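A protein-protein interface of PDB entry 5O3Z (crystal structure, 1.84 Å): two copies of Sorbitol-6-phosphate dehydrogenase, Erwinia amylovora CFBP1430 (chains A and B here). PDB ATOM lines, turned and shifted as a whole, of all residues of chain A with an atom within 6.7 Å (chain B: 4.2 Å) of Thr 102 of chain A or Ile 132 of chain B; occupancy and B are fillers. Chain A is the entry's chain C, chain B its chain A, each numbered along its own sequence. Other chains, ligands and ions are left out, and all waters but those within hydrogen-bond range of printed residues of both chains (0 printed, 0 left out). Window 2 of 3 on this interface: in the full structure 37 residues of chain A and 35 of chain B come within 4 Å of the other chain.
The backbone carbonyl oxygen of Phe 104 of chain A sits at hydrogen-bond distance from the guanidinium group of Arg 125 of chain B, 2.8 Å away.
No position is printed for both chains.
O of Ile 101 of chain A touches CG of Arg 125 of chain B, at 3.5 Å. CG2 of Ile 101 of chain A touches CD2 of Leu 176 of chain B, at 3.7 Å. O of Thr 102 of chain A touches CE of Lys 129 of chain B, 3.7 Å away. CD1 of Ile 132 of chain B touches OG1 of Thr 102 of chain A (3.9 Å).
Printed residues of chain B within 4 Å of Thr 102 of chain A: Lys 129 (3.7 Å) and Ile 132 (3.9 Å). Of the printed residues of chain A, Leu 176 of chain B touches Ile 101 (3.7 Å). Of the printed residues of chain B, Phe 104 of chain A touches Arg 125. Printed residues of chain B within 4 Å of Ile 101 of chain A: Arg 125 (3.5 Å) and Leu 176 (3.7 Å). Printed residues of chain A within 4 Å of Arg 125 of chain B: Ile 101 (3.5 Å) and Phe 104 (2.8 Å). Of the printed residues of chain A, Lys 129 of chain B touches Thr 102 (3.7 Å). Ala 99 of chain A touches none of the printed residues of chain B. The nearest residue of chain B that does not touch Thr 102 of chain A is Arg 125 of chain B (4.1 Å). The nearest residue of chain A that does not touch Ile 132 of chain B is Ile 101 of chain A (6.2 Å). The nearest printed residue of chain A that does not touch Leu 176 of chain B is Thr 102 of chain A (4.9 Å).
The side-chain hydroxyl (OG) of Ser 128 of chain B lies within hydrogen-bond range of the backbone carbonyl oxygen (O) of Arg 125 of chain B.
Of the 6 printed residues of chain A, 3 touch a printed residue of chain B. Hydrophobic or aromatic side chains of chain A that line the printed part of chain B: Ile 101. Among the printed residues, 5 pairs touch across the chains. Among the printed residues, no Asp or Glu carboxylate lies within 4 Å of a Lys or Arg side-chain nitrogen of the other chain.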
ATOM      1  N   ALA A  99       0.223 -25.665  33.926  1.00  0.00           N
ATOM      2  CA  ALA A  99      -0.825 -24.815  33.316  1.00  0.00           C
ATOM      3  C   ALA A  99      -0.942 -25.167  31.822  1.00  0.00           C
ATOM      4  O   ALA A  99       0.066 -25.485  31.206  1.00  0.00           O
ATOM      5  CB  ALA A  99      -0.474 -23.347  33.466  1.00  0.00           C
ATOM      6  N   PRO A 100      -2.169 -25.136  31.248  1.00  0.00           N
ATOM      7  CA  PRO A 100      -2.269 -25.271  29.788  1.00  0.00           C
ATOM      8  C   PRO A 100      -1.453 -24.200  29.124  1.00  0.00           C
ATOM      9  O   PRO A 100      -1.320 -23.101  29.682  1.00  0.00           O
ATOM     10  CB  PRO A 100      -3.761 -25.045  29.497  1.00  0.00           C
ATOM     11  CG  PRO A 100      -4.420 -24.663  30.811  1.00  0.00           C
ATOM     12  CD  PRO A 100      -3.509 -25.077  31.904  1.00  0.00           C
ATOM     13  N   ILE A 101      -0.871 -24.484  27.958  1.00  0.00           N
ATOM     14  CA  ILE A 101      -0.058 -23.482  27.308  1.00  0.00           C
ATOM     15  C   ILE A 101      -0.746 -22.129  27.258  1.00  0.00           C
ATOM     16  O   ILE A 101      -0.162 -21.086  27.570  1.00  0.00           O
ATOM     17  CB  ILE A 101       0.325 -23.894  25.874  1.00  0.00           C
ATOM     18  CG1 ILE A 101       1.124 -22.843  25.193  1.00  0.00           C
ATOM     19  CG2 ILE A 101      -0.874 -24.303  25.009  1.00  0.00           C
ATOM     20  CD1 ILE A 101       2.342 -22.387  25.982  1.00  0.00           C
ATOM     21  N   THR A 102      -2.019 -22.157  26.846  1.00  0.00           N
ATOM     22  CA  THR A 102      -2.916 -20.979  26.859  1.00  0.00           C
ATOM     23  C   THR A 102      -2.775 -20.003  28.083  1.00  0.00           C
ATOM     24  O   THR A 102      -2.867 -18.771  27.909  1.00  0.00           O
ATOM     25  CB  THR A 102      -4.375 -21.497  26.851  1.00  0.00           C
ATOM     26  OG1 THR A 102      -4.600 -22.271  25.666  1.00  0.00           O
ATOM     27  CG2 THR A 102      -5.388 -20.350  26.939  1.00  0.00           C
ATOM     28  N   GLN A 103      -2.590 -20.556  29.287  1.00  0.00           N
ATOM     29  CA  GLN A 103      -2.547 -19.782  30.524  1.00  0.00           C
ATOM     30  C   GLN A 103      -1.193 -19.879  31.231  1.00  0.00           C
ATOM     31  O   GLN A 103      -1.107 -19.515  32.385  1.00  0.00           O
ATOM     32  CB  GLN A 103      -3.660 -20.239  31.477  1.00  0.00           C
ATOM     33  CG  GLN A 103      -5.050 -20.212  30.843  1.00  0.00           C
ATOM     34  CD  GLN A 103      -5.999 -21.242  31.433  1.00  0.00           C
ATOM     35  OE1 GLN A 103      -5.858 -21.650  32.587  1.00  0.00           O
ATOM     36  NE2 GLN A 103      -6.972 -21.674  30.635  1.00  0.00           N
ATOM     37  N   PHE A 104      -0.135 -20.346  30.539  1.00  0.00           N
ATOM     38  CA  PHE A 104       1.163 -20.491  31.163  1.00  0.00           C
ATOM     39  C   PHE A 104       1.851 -19.155  31.192  1.00  0.00           C
ATOM     40  O   PHE A 104       1.969 -18.506  30.152  1.00  0.00           O
ATOM     41  CB  PHE A 104       2.048 -21.507  30.386  1.00  0.00           C
ATOM     42  CG  PHE A 104       3.036 -22.231  31.261  1.00  0.00           C
ATOM     43  CD1 PHE A 104       4.228 -21.655  31.588  1.00  0.00           C
ATOM     44  CD2 PHE A 104       2.768 -23.513  31.738  1.00  0.00           C
ATOM     45  CE1 PHE A 104       5.160 -22.333  32.376  1.00  0.00           C
ATOM     46  CE2 PHE A 104       3.701 -24.213  32.490  1.00  0.00           C
ATOM     47  CZ  PHE A 104       4.880 -23.599  32.854  1.00  0.00           C
ATOM     48  N   ARG B 125       1.956 -19.765  22.217  1.00  0.00           N
ATOM     49  CA  ARG B 125       0.919 -19.334  23.147  1.00  0.00           C
ATOM     50  C   ARG B 125      -0.103 -18.436  22.482  1.00  0.00           C
ATOM     51  O   ARG B 125      -1.304 -18.695  22.569  1.00  0.00           O
ATOM     52  CB  ARG B 125       1.488 -18.581  24.372  1.00  0.00           C
ATOM     53  CG  ARG B 125       0.413 -18.398  25.459  1.00  0.00           C
ATOM     54  CD  ARG B 125       0.965 -17.827  26.738  1.00  0.00           C
ATOM     55  NE  ARG B 125       1.368 -16.430  26.564  1.00  0.00           N
ATOM     56  CZ  ARG B 125       2.104 -15.741  27.432  1.00  0.00           C
ATOM     57  NH1 ARG B 125       2.588 -16.321  28.547  1.00  0.00           N
ATOM     58  NH2 ARG B 125       2.384 -14.478  27.173  1.00  0.00           N
ATOM     59  N   SER B 128      -1.812 -20.027  19.142  1.00  0.00           N
ATOM     60  CA  SER B 128      -2.799 -21.031  19.572  1.00  0.00           C
ATOM     61  C   SER B 128      -4.109 -20.472  20.097  1.00  0.00           C
ATOM     62  O   SER B 128      -5.176 -21.068  19.843  1.00  0.00           O
ATOM     63  CB  SER B 128      -2.257 -22.022  20.613  1.00  0.00           C
ATOM     64  OG  SER B 128      -1.833 -21.451  21.837  1.00  0.00           O
ATOM     65  N   LYS B 129      -4.075 -19.374  20.865  1.00  0.00           N
ATOM     66  CA  LYS B 129      -5.319 -18.770  21.371  1.00  0.00           C
ATOM     67  C   LYS B 129      -6.217 -18.345  20.204  1.00  0.00           C
ATOM     68  O   LYS B 129      -7.433 -18.555  20.242  1.00  0.00           O
ATOM     69  CB  LYS B 129      -5.028 -17.506  22.194  1.00  0.00           C
ATOM     70  CG  LYS B 129      -4.411 -17.746  23.548  1.00  0.00           C
ATOM     71  CD  LYS B 129      -3.600 -16.503  23.945  1.00  0.00           C
ATOM     72  CE  LYS B 129      -3.632 -16.207  25.417  1.00  0.00           C
ATOM     73  NZ  LYS B 129      -4.893 -15.507  25.751  1.00  0.00           N
ATOM     74  N   LEU B 130      -5.627 -17.750  19.188  1.00  0.00           N
ATOM     75  CA  LEU B 130      -6.391 -17.336  17.980  1.00  0.00           C
ATOM     76  C   LEU B 130      -6.994 -18.544  17.287  1.00  0.00           C
ATOM     77  O   LEU B 130      -8.123 -18.473  16.723  1.00  0.00           O
ATOM     78  CB  LEU B 130      -5.539 -16.516  16.991  1.00  0.00           C
ATOM     79  CG  LEU B 130      -5.106 -15.085  17.426  1.00  0.00           C
ATOM     80  CD1 LEU B 130      -4.237 -14.410  16.346  1.00  0.00           C
ATOM     81  CD2 LEU B 130      -6.293 -14.193  17.742  1.00  0.00           C
ATOM     82  N   MET B 131      -6.263 -19.661  17.305  1.00  0.00           N
ATOM     83  CA  MET B 131      -6.678 -20.851  16.567  1.00  0.00           C
ATOM     84  C   MET B 131      -7.833 -21.476  17.301  1.00  0.00           C
ATOM     85  O   MET B 131      -8.801 -21.935  16.679  1.00  0.00           O
ATOM     86  CB  MET B 131      -5.510 -21.859  16.457  1.00  0.00           C
ATOM     87  CG  MET B 131      -4.570 -21.549  15.363  1.00  0.00           C
ATOM     88  SD  MET B 131      -3.097 -22.601  15.554  1.00  0.00           S
ATOM     89  CE  MET B 131      -1.937 -21.790  14.487  1.00  0.00           C
ATOM     90  N   ILE B 132      -7.724 -21.497  18.620  1.00  0.00           N
ATOM     91  CA  ILE B 132      -8.753 -21.963  19.505  1.00  0.00           C
ATOM     92  C   ILE B 132     -10.029 -21.147  19.437  1.00  0.00           C
ATOM     93  O   ILE B 132     -11.141 -21.715  19.342  1.00  0.00           O
ATOM     94  CB  ILE B 132      -8.245 -22.011  20.959  1.00  0.00           C
ATOM     95  CG1 ILE B 132      -7.231 -23.164  21.064  1.00  0.00           C
ATOM     96  CG2 ILE B 132      -9.355 -22.243  21.984  1.00  0.00           C
ATOM     97  CD1 ILE B 132      -6.356 -23.065  22.290  1.00  0.00           C
ATOM     98  N   ARG B 133      -9.873 -19.839  19.469  1.00  0.00           N
ATOM     99  CA  ARG B 133     -11.016 -18.908  19.448  1.00  0.00           C
ATOM    100  C   ARG B 133     -11.876 -19.141  18.242  1.00  0.00           C
ATOM    101  O   ARG B 133     -13.057 -19.272  18.384  1.00  0.00           O
ATOM    102  CB  ARG B 133     -10.531 -17.458  19.395  1.00  0.00           C
ATOM    103  CG  ARG B 133     -11.652 -16.416  19.560  1.00  0.00           C
ATOM    104  CD  ARG B 133     -11.177 -15.044  19.094  1.00  0.00           C
ATOM    105  NE  ARG B 133     -10.910 -15.007  17.657  1.00  0.00           N
ATOM    106  CZ  ARG B 133     -10.175 -14.081  17.018  1.00  0.00           C
ATOM    107  NH1 ARG B 133      -9.623 -13.078  17.681  1.00  0.00           N
ATOM    108  NH2 ARG B 133      -9.982 -14.150  15.701  1.00  0.00           N
ATOM    109  N   ASP B 134     -11.248 -19.196  17.075  1.00  0.00           N
ATOM    110  CA  ASP B 134     -11.940 -19.369  15.788  1.00  0.00           C
ATOM    111  C   ASP B 134     -12.194 -20.788  15.366  1.00  0.00           C
ATOM    112  O   ASP B 134     -12.529 -21.013  14.218  1.00  0.00           O
ATOM    113  CB  ASP B 134     -11.109 -18.728  14.664  1.00  0.00           C
ATOM    114  CG  ASP B 134     -11.136 -17.213  14.713  1.00  0.00           C
ATOM    115  OD1 ASP B 134     -11.956 -16.717  15.523  1.00  0.00           O
ATOM    116  OD2 ASP B 134     -10.353 -16.544  13.962  1.00  0.00           O
ATOM    117  N   GLY B 135     -12.003 -21.760  16.241  1.00  0.00           N
ATOM    118  CA  GLY B 135     -12.184 -23.184  15.860  1.00  0.00           C
ATOM    119  C   GLY B 135     -11.357 -23.780  14.716  1.00  0.00           C
ATOM    120  O   GLY B 135     -11.833 -24.641  13.987  1.00  0.00           O
ATOM    121  N   LEU B 176      -2.665 -29.223  22.953  1.00  0.00           N
ATOM    122  CA  LEU B 176      -3.495 -28.682  21.878  1.00  0.00           C
ATOM    123  C   LEU B 176      -4.227 -29.726  21.058  1.00  0.00           C
ATOM    124  O   LEU B 176      -5.145 -29.357  20.283  1.00  0.00           O
ATOM    125  CB  LEU B 176      -2.696 -27.713  21.017  1.00  0.00           C
ATOM    126  CG  LEU B 176      -2.054 -26.550  21.770  1.00  0.00           C
ATOM    127  CD1 LEU B 176      -1.166 -25.725  20.853  1.00  0.00           C
ATOM    128  CD2 LEU B 176      -3.123 -25.604  22.345  1.00  0.00           C
ATOM    129  N   TYR B 179      -7.935 -29.600  20.555  1.00  0.00           N
ATOM    130  CA  TYR B 179      -8.400 -28.577  19.607  1.00  0.00           C
ATOM    131  C   TYR B 179      -8.059 -28.877  18.158  1.00  0.00           C
ATOM    132  O   TYR B 179      -8.272 -28.030  17.300  1.00  0.00           O
ATOM    133  CB  TYR B 179      -7.778 -27.228  19.969  1.00  0.00           C
ATOM    134  CG  TYR B 179      -8.028 -26.809  21.361  1.00  0.00           C
ATOM    135  CD1 TYR B 179      -9.328 -26.431  21.790  1.00  0.00           C
ATOM    136  CD2 TYR B 179      -6.999 -26.740  22.275  1.00  0.00           C
ATOM    137  CE1 TYR B 179      -9.571 -26.015  23.075  1.00  0.00           C
ATOM    138  CE2 TYR B 179      -7.230 -26.295  23.566  1.00  0.00           C
ATOM    139  CZ  TYR B 179      -8.528 -25.944  23.947  1.00  0.00           C
ATOM    140  OH  TYR B 179      -8.710 -25.572  25.233  1.00  0.00           O
